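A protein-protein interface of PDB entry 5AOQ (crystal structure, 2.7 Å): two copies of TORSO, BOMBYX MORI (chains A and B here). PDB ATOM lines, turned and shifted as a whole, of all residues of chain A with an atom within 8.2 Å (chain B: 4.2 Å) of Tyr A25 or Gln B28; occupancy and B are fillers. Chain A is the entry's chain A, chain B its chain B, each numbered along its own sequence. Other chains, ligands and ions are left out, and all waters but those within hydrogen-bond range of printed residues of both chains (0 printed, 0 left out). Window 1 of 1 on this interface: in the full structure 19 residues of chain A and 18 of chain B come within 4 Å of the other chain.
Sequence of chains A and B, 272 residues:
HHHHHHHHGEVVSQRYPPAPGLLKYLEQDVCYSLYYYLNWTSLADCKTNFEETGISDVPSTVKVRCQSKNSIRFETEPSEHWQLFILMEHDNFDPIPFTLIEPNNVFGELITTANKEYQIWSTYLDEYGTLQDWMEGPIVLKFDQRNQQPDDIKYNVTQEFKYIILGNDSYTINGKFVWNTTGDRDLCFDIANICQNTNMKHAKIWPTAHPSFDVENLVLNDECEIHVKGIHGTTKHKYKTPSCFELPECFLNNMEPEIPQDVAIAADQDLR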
ATOM      1  N   ALA A  19      20.249  -2.378  12.024  1.00  0.00           N
ATOM      2  CA  ALA A  19      19.537  -1.260  11.417  1.00  0.00           C
ATOM      3  C   ALA A  19      20.437  -0.024  11.414  1.00  0.00           C
ATOM      4  O   ALA A  19      20.582   0.635  12.442  1.00  0.00           O
ATOM      5  CB  ALA A  19      18.247  -0.982  12.167  1.00  0.00           C
ATOM      6  N   PRO A  20      21.048   0.294  10.257  1.00  0.00           N
ATOM      7  CA  PRO A  20      21.963   1.439  10.192  1.00  0.00           C
ATOM      8  C   PRO A  20      21.263   2.767  10.449  1.00  0.00           C
ATOM      9  O   PRO A  20      21.871   3.682  11.008  1.00  0.00           O
ATOM     10  CB  PRO A  20      22.501   1.381   8.756  1.00  0.00           C
ATOM     11  CG  PRO A  20      22.237  -0.009   8.291  1.00  0.00           C
ATOM     12  CD  PRO A  20      20.981  -0.424   8.972  1.00  0.00           C
ATOM     13  N   GLY A  21      19.997   2.857  10.060  1.00  0.00           N
ATOM     14  CA  GLY A  21      19.229   4.077  10.229  1.00  0.00           C
ATOM     15  C   GLY A  21      19.081   4.460  11.688  1.00  0.00           C
ATOM     16  O   GLY A  21      18.832   5.624  12.011  1.00  0.00           O
ATOM     17  N   LEU A  22      19.235   3.473  12.566  1.00  0.00           N
ATOM     18  CA  LEU A  22      19.154   3.685  14.006  1.00  0.00           C
ATOM     19  C   LEU A  22      20.538   3.582  14.640  1.00  0.00           C
ATOM     20  O   LEU A  22      20.901   4.393  15.490  1.00  0.00           O
ATOM     21  CB  LEU A  22      18.205   2.668  14.630  1.00  0.00           C
ATOM     22  CG  LEU A  22      16.782   2.689  14.076  1.00  0.00           C
ATOM     23  CD1 LEU A  22      16.024   1.476  14.560  1.00  0.00           C
ATOM     24  CD2 LEU A  22      16.059   3.959  14.473  1.00  0.00           C
ATOM     25  N   LEU A  23      21.301   2.576  14.223  1.00  0.00           N
ATOM     26  CA  LEU A  23      22.681   2.409  14.673  1.00  0.00           C
ATOM     27  C   LEU A  23      23.513   3.654  14.385  1.00  0.00           C
ATOM     28  O   LEU A  23      24.516   3.911  15.052  1.00  0.00           O
ATOM     29  CB  LEU A  23      23.321   1.196  13.998  1.00  0.00           C
ATOM     30  CG  LEU A  23      22.861  -0.177  14.485  1.00  0.00           C
ATOM     31  CD1 LEU A  23      23.357  -1.260  13.548  1.00  0.00           C
ATOM     32  CD2 LEU A  23      23.364  -0.430  15.897  1.00  0.00           C
ATOM     33  N   LYS A  24      23.089   4.413  13.380  1.00  0.00           N
ATOM     34  CA  LYS A  24      23.706   5.692  13.038  1.00  0.00           C
ATOM     35  C   LYS A  24      23.890   6.614  14.245  1.00  0.00           C
ATOM     36  O   LYS A  24      24.774   7.472  14.245  1.00  0.00           O
ATOM     37  CB  LYS A  24      22.855   6.388  11.968  1.00  0.00           C
ATOM     38  CG  LYS A  24      22.754   7.902  12.085  1.00  0.00           C
ATOM     39  CD  LYS A  24      21.904   8.468  10.962  1.00  0.00           C
ATOM     40  CE  LYS A  24      21.656   9.955  11.137  1.00  0.00           C
ATOM     41  NZ  LYS A  24      20.758  10.487  10.074  1.00  0.00           N
ATOM     42  N   TYR A  25      23.063   6.433  15.270  1.00  0.00           N
ATOM     43  CA  TYR A  25      23.041   7.350  16.408  1.00  0.00           C
ATOM     44  C   TYR A  25      23.958   6.929  17.560  1.00  0.00           C
ATOM     45  O   TYR A  25      24.074   7.645  18.552  1.00  0.00           O
ATOM     46  CB  TYR A  25      21.607   7.503  16.917  1.00  0.00           C
ATOM     47  CG  TYR A  25      20.696   8.146  15.899  1.00  0.00           C
ATOM     48  CD1 TYR A  25      20.750   9.512  15.661  1.00  0.00           C
ATOM     49  CD2 TYR A  25      19.792   7.389  15.167  1.00  0.00           C
ATOM     50  CE1 TYR A  25      19.928  10.108  14.729  1.00  0.00           C
ATOM     51  CE2 TYR A  25      18.963   7.977  14.231  1.00  0.00           C
ATOM     52  CZ  TYR A  25      19.035   9.336  14.017  1.00  0.00           C
ATOM     53  OH  TYR A  25      18.214   9.928  13.087  1.00  0.00           O
ATOM     54  N   LEU A  26      24.607   5.776  17.426  1.00  0.00           N
ATOM     55  CA  LEU A  26      25.561   5.318  18.432  1.00  0.00           C
ATOM     56  C   LEU A  26      26.958   5.884  18.175  1.00  0.00           C
ATOM     57  O   LEU A  26      27.894   5.645  18.947  1.00  0.00           O
ATOM     58  CB  LEU A  26      25.612   3.789  18.460  1.00  0.00           C
ATOM     59  CG  LEU A  26      24.267   3.082  18.642  1.00  0.00           C
ATOM     60  CD1 LEU A  26      24.465   1.574  18.708  1.00  0.00           C
ATOM     61  CD2 LEU A  26      23.540   3.587  19.883  1.00  0.00           C
ATOM     62  N   GLU A  27      27.092   6.644  17.092  1.00  0.00           N
ATOM     63  CA  GLU A  27      28.388   7.169  16.680  1.00  0.00           C
ATOM     64  C   GLU A  27      28.979   8.096  17.736  1.00  0.00           C
ATOM     65  O   GLU A  27      30.190   8.095  17.948  1.00  0.00           O
ATOM     66  CB  GLU A  27      28.268   7.902  15.342  1.00  0.00           C
ATOM     67  CG  GLU A  27      27.941   6.986  14.171  1.00  0.00           C
ATOM     68  CD  GLU A  27      27.832   7.732  12.853  1.00  0.00           C
ATOM     69  OE1 GLU A  27      28.153   8.939  12.823  1.00  0.00           O
ATOM     70  OE2 GLU A  27      27.431   7.107  11.847  1.00  0.00           O
ATOM     71  N   GLN A  28      28.132   8.875  18.400  1.00  0.00           N
ATOM     72  CA  GLN A  28      28.599   9.751  19.469  1.00  0.00           C
ATOM     73  C   GLN A  28      29.229   8.914  20.578  1.00  0.00           C
ATOM     74  O   GLN A  28      30.352   9.175  21.005  1.00  0.00           O
ATOM     75  CB  GLN A  28      27.453  10.596  20.035  1.00  0.00           C
ATOM     76  CG  GLN A  28      27.877  11.533  21.165  1.00  0.00           C
ATOM     77  CD  GLN A  28      26.710  12.274  21.789  1.00  0.00           C
ATOM     78  OE1 GLN A  28      25.660  12.442  21.169  1.00  0.00           O
ATOM     79  NE2 GLN A  28      26.891  12.725  23.025  1.00  0.00           N
ATOM     80  N   ASP A  29      28.495   7.902  21.028  1.00  0.00           N
ATOM     81  CA  ASP A  29      28.969   7.003  22.074  1.00  0.00           C
ATOM     82  C   ASP A  29      30.296   6.359  21.684  1.00  0.00           C
ATOM     83  O   ASP A  29      31.285   6.442  22.423  1.00  0.00           O
ATOM     84  CB  ASP A  29      27.927   5.919  22.352  1.00  0.00           C
ATOM     85  CG  ASP A  29      26.608   6.488  22.844  1.00  0.00           C
ATOM     86  OD1 ASP A  29      26.626   7.345  23.752  1.00  0.00           O
ATOM     87  OD2 ASP A  29      25.552   6.076  22.320  1.00  0.00           O
ATOM     88  N   VAL A  30      30.313   5.728  20.514  1.00  0.00           N
ATOM     89  CA  VAL A  30      31.505   5.029  20.041  1.00  0.00           C
ATOM     90  C   VAL A  30      32.678   5.992  19.879  1.00  0.00           C
ATOM     91  O   VAL A  30      33.814   5.654  20.205  1.00  0.00           O
ATOM     92  CB  VAL A  30      31.247   4.306  18.699  1.00  0.00           C
ATOM     93  CG1 VAL A  30      32.533   3.674  18.162  1.00  0.00           C
ATOM     94  CG2 VAL A  30      30.171   3.246  18.867  1.00  0.00           C
ATOM     95  N   TYR A  32      33.136   8.985  21.389  1.00  0.00           N
ATOM     96  CA  TYR A  32      33.581   9.443  22.703  1.00  0.00           C
ATOM     97  C   TYR A  32      34.425   8.374  23.388  1.00  0.00           C
ATOM     98  O   TYR A  32      35.574   8.621  23.756  1.00  0.00           O
ATOM     99  CB  TYR A  32      32.389   9.811  23.591  1.00  0.00           C
ATOM    100  CG  TYR A  32      31.797  11.181  23.324  1.00  0.00           C
ATOM    101  CD1 TYR A  32      31.588  11.636  22.029  1.00  0.00           C
ATOM    102  CD2 TYR A  32      31.438  12.015  24.375  1.00  0.00           C
ATOM    103  CE1 TYR A  32      31.043  12.885  21.789  1.00  0.00           C
ATOM    104  CE2 TYR A  32      30.894  13.265  24.144  1.00  0.00           C
ATOM    105  CZ  TYR A  32      30.698  13.694  22.850  1.00  0.00           C
ATOM    106  OH  TYR A  32      30.156  14.936  22.615  1.00  0.00           O
ATOM    107  N   PHE A  50      28.072   3.847  10.639  1.00  0.00           N
ATOM    108  CA  PHE A  50      27.252   2.642  10.717  1.00  0.00           C
ATOM    109  C   PHE A  50      26.499   2.371   9.419  1.00  0.00           C
ATOM    110  O   PHE A  50      26.054   1.250   9.176  1.00  0.00           O
ATOM    111  CB  PHE A  50      26.254   2.749  11.869  1.00  0.00           C
ATOM    112  CG  PHE A  50      26.862   2.524  13.221  1.00  0.00           C
ATOM    113  CD1 PHE A  50      26.944   1.248  13.749  1.00  0.00           C
ATOM    114  CD2 PHE A  50      27.349   3.584  13.966  1.00  0.00           C
ATOM    115  CE1 PHE A  50      27.498   1.032  14.993  1.00  0.00           C
ATOM    116  CE2 PHE A  50      27.906   3.374  15.212  1.00  0.00           C
ATOM    117  CZ  PHE A  50      27.980   2.096  15.725  1.00  0.00           C
ATOM    118  N   GLU A  51      26.360   3.400   8.591  1.00  0.00           N
ATOM    119  CA  GLU A  51      25.597   3.289   7.355  1.00  0.00           C
ATOM    120  C   GLU A  51      26.467   2.785   6.204  1.00  0.00           C
ATOM    121  O   GLU A  51      25.951   2.385   5.162  1.00  0.00           O
ATOM    122  CB  GLU A  51      24.965   4.640   7.013  1.00  0.00           C
ATOM    123  CG  GLU A  51      23.807   5.002   7.940  1.00  0.00           C
ATOM    124  CD  GLU A  51      23.225   6.374   7.662  1.00  0.00           C
ATOM    125  OE1 GLU A  51      24.001   7.350   7.608  1.00  0.00           O
ATOM    126  OE2 GLU A  51      21.989   6.475   7.508  1.00  0.00           O
ATOM    127  N   PHE A  93      12.396   0.634  17.184  1.00  0.00           N
ATOM    128  CA  PHE A  93      11.893   1.994  17.329  1.00  0.00           C
ATOM    129  C   PHE A  93      12.729   2.740  18.355  1.00  0.00           C
ATOM    130  O   PHE A  93      13.207   3.847  18.109  1.00  0.00           O
ATOM    131  CB  PHE A  93      10.424   1.981  17.759  1.00  0.00           C
ATOM    132  CG  PHE A  93       9.507   1.319  16.769  1.00  0.00           C
ATOM    133  CD1 PHE A  93       9.711   1.461  15.407  1.00  0.00           C
ATOM    134  CD2 PHE A  93       8.435   0.556  17.203  1.00  0.00           C
ATOM    135  CE1 PHE A  93       8.866   0.854  14.497  1.00  0.00           C
ATOM    136  CE2 PHE A  93       7.588  -0.054  16.299  1.00  0.00           C
ATOM    137  CZ  PHE A  93       7.804   0.095  14.945  1.00  0.00           C
ATOM    138  N   ASP A  94      12.906   2.106  19.509  1.00  0.00           N
ATOM    139  CA  ASP A  94      13.702   2.664  20.592  1.00  0.00           C
ATOM    140  C   ASP A  94      15.194   2.631  20.269  1.00  0.00           C
ATOM    141  O   ASP A  94      15.618   1.899  19.374  1.00  0.00           O
ATOM    142  CB  ASP A  94      13.430   1.894  21.885  1.00  0.00           C
ATOM    143  CG  ASP A  94      11.973   1.949  22.296  1.00  0.00           C
ATOM    144  OD1 ASP A  94      11.267   2.889  21.874  1.00  0.00           O
ATOM    145  OD2 ASP A  94      11.531   1.048  23.042  1.00  0.00           O
ATOM    146  N   PRO A  95      15.992   3.435  20.991  1.00  0.00           N
ATOM    147  CA  PRO A  95      17.450   3.388  20.837  1.00  0.00           C
ATOM    148  C   PRO A  95      17.998   1.986  21.081  1.00  0.00           C
ATOM    149  O   PRO A  95      17.482   1.248  21.920  1.00  0.00           O
ATOM    150  CB  PRO A  95      17.955   4.382  21.894  1.00  0.00           C
ATOM    151  CG  PRO A  95      16.780   4.661  22.781  1.00  0.00           C
ATOM    152  CD  PRO A  95      15.581   4.497  21.922  1.00  0.00           C
ATOM    153  N   ILE A  96      19.044   1.635  20.344  1.00  0.00           N
ATOM    154  CA  ILE A  96      19.582   0.279  20.342  1.00  0.00           C
ATOM    155  C   ILE A  96      20.513   0.005  21.527  1.00  0.00           C
ATOM    156  O   ILE A  96      21.477   0.742  21.736  1.00  0.00           O
ATOM    157  CB  ILE A  96      20.354   0.006  19.042  1.00  0.00           C
ATOM    158  CG1 ILE A  96      19.494   0.359  17.828  1.00  0.00           C
ATOM    159  CG2 ILE A  96      20.774  -1.458  18.967  1.00  0.00           C
ATOM    160  CD1 ILE A  96      20.275   0.456  16.557  1.00  0.00           C
ATOM    161  N   PHE A  98      23.609  -1.427  23.409  1.00  0.00           N
ATOM    162  CA  PHE A  98      24.941  -1.750  22.916  1.00  0.00           C
ATOM    163  C   PHE A  98      25.982  -1.756  24.026  1.00  0.00           C
ATOM    164  O   PHE A  98      25.735  -1.258  25.125  1.00  0.00           O
ATOM    165  CB  PHE A  98      25.359  -0.748  21.839  1.00  0.00           C
ATOM    166  CG  PHE A  98      25.799   0.577  22.392  1.00  0.00           C
ATOM    167  CD1 PHE A  98      24.870   1.557  22.694  1.00  0.00           C
ATOM    168  CD2 PHE A  98      27.141   0.839  22.618  1.00  0.00           C
ATOM    169  CE1 PHE A  98      25.269   2.777  23.207  1.00  0.00           C
ATOM    170  CE2 PHE A  98      27.546   2.056  23.132  1.00  0.00           C
ATOM    171  CZ  PHE A  98      26.608   3.026  23.427  1.00  0.00           C
ATOM    172  N   LEU B  26      25.929  15.961  17.885  1.00  0.00           N
ATOM    173  CA  LEU B  26      24.795  16.336  18.729  1.00  0.00           C
ATOM    174  C   LEU B  26      23.485  15.740  18.214  1.00  0.00           C
ATOM    175  O   LEU B  26      22.424  15.918  18.823  1.00  0.00           O
ATOM    176  CB  LEU B  26      24.668  17.858  18.811  1.00  0.00           C
ATOM    177  CG  LEU B  26      25.919  18.616  19.258  1.00  0.00           C
ATOM    178  CD1 LEU B  26      25.633  20.108  19.345  1.00  0.00           C
ATOM    179  CD2 LEU B  26      26.430  18.088  20.591  1.00  0.00           C
ATOM    180  N   GLU B  27      23.565  15.029  17.094  1.00  0.00           N
ATOM    181  CA  GLU B  27      22.377  14.494  16.440  1.00  0.00           C
ATOM    182  C   GLU B  27      21.648  13.494  17.331  1.00  0.00           C
ATOM    183  O   GLU B  27      20.418  13.455  17.344  1.00  0.00           O
ATOM    184  CB  GLU B  27      22.759  13.846  15.106  1.00  0.00           C
ATOM    185  CG  GLU B  27      23.271  14.848  14.079  1.00  0.00           C
ATOM    186  CD  GLU B  27      23.645  14.203  12.761  1.00  0.00           C
ATOM    187  OE1 GLU B  27      23.374  12.996  12.587  1.00  0.00           O
ATOM    188  OE2 GLU B  27      24.209  14.907  11.895  1.00  0.00           O
ATOM    189  N   GLN B  28      22.403  12.696  18.081  1.00  0.00           N
ATOM    190  CA  GLN B  28      21.808  11.753  19.022  1.00  0.00           C
ATOM    191  C   GLN B  28      20.987  12.502  20.059  1.00  0.00           C
ATOM    192  O   GLN B  28      19.829  12.171  20.305  1.00  0.00           O
ATOM    193  CB  GLN B  28      22.882  10.913  19.718  1.00  0.00           C
ATOM    194  CG  GLN B  28      22.328   9.928  20.742  1.00  0.00           C
ATOM    195  CD  GLN B  28      23.418   9.198  21.501  1.00  0.00           C
ATOM    196  OE1 GLN B  28      24.541   9.062  21.020  1.00  0.00           O
ATOM    197  NE2 GLN B  28      23.096   8.743  22.706  1.00  0.00           N
ATOM    198  N   ASP B  29      21.604  13.506  20.670  1.00  0.00           N
ATOM    199  CA  ASP B  29      20.936  14.328  21.669  1.00  0.00           C
ATOM    200  C   ASP B  29      19.671  14.968  21.108  1.00  0.00           C
ATOM    201  O   ASP B  29      18.585  14.810  21.672  1.00  0.00           O
ATOM    202  CB  ASP B  29      21.890  15.407  22.188  1.00  0.00           C
ATOM    203  CG  ASP B  29      23.105  14.823  22.888  1.00  0.00           C
ATOM    204  OD1 ASP B  29      22.929  13.920  23.731  1.00  0.00           O
ATOM    205  OD2 ASP B  29      24.235  15.267  22.593  1.00  0.00           O
ATOM    206  N   VAL B  30      19.809  15.682  19.993  1.00  0.00           N
ATOM    207  CA  VAL B  30      18.669  16.380  19.403  1.00  0.00           C
ATOM    208  C   VAL B  30      17.563  15.416  18.978  1.00  0.00           C
ATOM    209  O   VAL B  30      16.385  15.684  19.201  1.00  0.00           O
ATOM    210  CB  VAL B  30      19.089  17.217  18.174  1.00  0.00           C
ATOM    211  CG1 VAL B  30      17.866  17.858  17.510  1.00  0.00           C
ATOM    212  CG2 VAL B  30      20.090  18.286  18.572  1.00  0.00           C
ATOM    213  N   CYS B  31      17.939  14.294  18.376  1.00  0.00           N
ATOM    214  CA  CYS B  31      16.951  13.351  17.863  1.00  0.00           C
ATOM    215  C   CYS B  31      16.279  12.583  18.998  1.00  0.00           C
ATOM    216  O   CYS B  31      15.082  12.300  18.936  1.00  0.00           O
ATOM    217  CB  CYS B  31      17.594  12.386  16.866  1.00  0.00           C
ATOM    218  SG  CYS B  31      18.003  13.165  15.280  1.00  0.00           S
ATOM    219  N   TYR B  32      17.047  12.244  20.030  1.00  0.00           N
ATOM    220  CA  TYR B  32      16.485  11.596  21.211  1.00  0.00           C
ATOM    221  C   TYR B  32      15.505  12.536  21.898  1.00  0.00           C
ATOM    222  O   TYR B  32      14.347  12.187  22.121  1.00  0.00           O
ATOM    223  CB  TYR B  32      17.582  11.191  22.199  1.00  0.00           C
ATOM    224  CG  TYR B  32      18.343   9.931  21.842  1.00  0.00           C
ATOM    225  CD1 TYR B  32      18.204   9.332  20.599  1.00  0.00           C
ATOM    226  CD2 TYR B  32      19.201   9.340  22.759  1.00  0.00           C
ATOM    227  CE1 TYR B  32      18.901   8.181  20.281  1.00  0.00           C
ATOM    228  CE2 TYR B  32      19.899   8.191  22.448  1.00  0.00           C
ATOM    229  CZ  TYR B  32      19.745   7.616  21.209  1.00  0.00           C
ATOM    230  OH  TYR B  32      20.441   6.472  20.894  1.00  0.00           O
ATOM    231  N   LEU B  43      13.008   6.268  15.582  1.00  0.00           N
ATOM    232  CA  LEU B  43      14.067   7.256  15.751  1.00  0.00           C
ATOM    233  C   LEU B  43      14.678   7.655  14.409  1.00  0.00           C
ATOM    234  O   LEU B  43      15.161   8.777  14.250  1.00  0.00           O
ATOM    235  CB  LEU B  43      15.151   6.700  16.679  1.00  0.00           C
ATOM    236  CG  LEU B  43      16.430   7.519  16.860  1.00  0.00           C
ATOM    237  CD1 LEU B  43      16.165   8.790  17.653  1.00  0.00           C
ATOM    238  CD2 LEU B  43      17.493   6.665  17.526  1.00  0.00           C
ATOM    239  N   ALA B  44      14.651   6.734  13.451  1.00  0.00           N
ATOM    240  CA  ALA B  44      15.307   6.932  12.159  1.00  0.00           C
ATOM    241  C   ALA B  44      14.727   8.108  11.376  1.00  0.00           C
ATOM    242  O   ALA B  44      15.420   8.729  10.570  1.00  0.00           O
ATOM    243  CB  ALA B  44      15.213   5.660  11.330  1.00  0.00           C
ATOM    244  N   CYS B  46      14.204  11.014  12.041  1.00  0.00           N
ATOM    245  CA  CYS B  46      14.619  12.315  12.554  1.00  0.00           C
ATOM    246  C   CYS B  46      15.158  13.205  11.437  1.00  0.00           C
ATOM    247  O   CYS B  46      14.708  14.336  11.264  1.00  0.00           O
ATOM    248  CB  CYS B  46      15.682  12.133  13.642  1.00  0.00           C
ATOM    249  SG  CYS B  46      16.195  13.646  14.482  1.00  0.00           S
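O of Tyr A25 sits close to OE1 of Gln B28 (2.9 Å).
O of Leu B43 sits at hydrogen-bond distance from OH of Tyr A25 (3.5 Å).
OE1 of Gln A28 lies close to OD2 of Asp B29, at 3.5 Å.
The side-chain carboxylate of Asp A29 sits close to the side-chain amide oxygen of Gln B28 (3.4 Å).
SG of Cys B46 forms a disulfide with SG of Cys B31.
Gly A21 touches Ala B44.
CB of Leu B43 touches CD2 of Leu A22, at 3.6 Å.
Ala B44 touches Leu A22.
Lys A24 touches Glu B27 (CE to OE1, 3.8 Å).
Cys B31 touches Tyr A25 (SG to CE1, 3.7 Å).
O of Ala B44 touches OH of Tyr A25, 3.9 Å away.
CB of Cys B46 touches OH of Tyr A25 (3.4 Å).
Gln B28 touches Gln A28.
Phe A93 touches Leu B43 (O to N, 3.5 Å).
Tyr B32 touches Pro A95.
Of the printed residues of chain B, Leu A22 touches Leu B43 and Ala B44.
Of the printed residues of chain B, Lys A24 touches Glu B27.
Glu A27 touches none of the printed residues of chain B.
Of the printed residues of chain B, Phe A93 touches Leu B43 (3.5 Å).
Phe A98 touches none of the printed residues of chain B.
Of chain A, only Tyr A25 (2.9 Å), Gln A28 (3.4 Å) and Asp A29 (3.4 Å) come within 4 Å of Gln B28.
Of the printed residues of chain A, Tyr B32 touches Pro A95.
Of the printed residues of chain A, Ala B44 touches Gly A21 (3.7 Å), Leu A22 (3.3 Å) and Tyr A25 (3.9 Å).
The nearest printed residue of chain B that does not touch Tyr A25 is Tyr B32 (4.3 Å).
The nearest residue of chain A that does not touch Gln B28 is Leu A26 (4.7 Å).
The nearest printed residue of chain A that does not touch Cys B46 is Lys A24 (6.4 Å).
Of the 10 printed residues of chain B, 8 touch a printed residue of chain A.
Printed residues of chain B that touch a printed residue of chain A: Glu B27, Gln B28, Asp B29, Cys B31, Tyr B32, Leu B43, Ala B44 and Cys B46.
Of the 20 printed residues of chain A, 8 touch a printed residue of chain B.
Hydrophobic or aromatic side chains of chain A within 4 Å of the printed part of chain B: Leu A22, Tyr A25 and Pro A95.
Among the printed residues, 14 pairs touch across the chains.
Among the printed residues, no Asp or Glu carboxylate lies within 4 Å of a Lys or Arg side-chain nitrogen of the other chain.
Gln A28 touches its own counterpart, Gln B28.
Gln A28 touches Asp B29, and with the chains exchanged Asp A29 touches Gln B28.
6 positions are printed for both chains.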
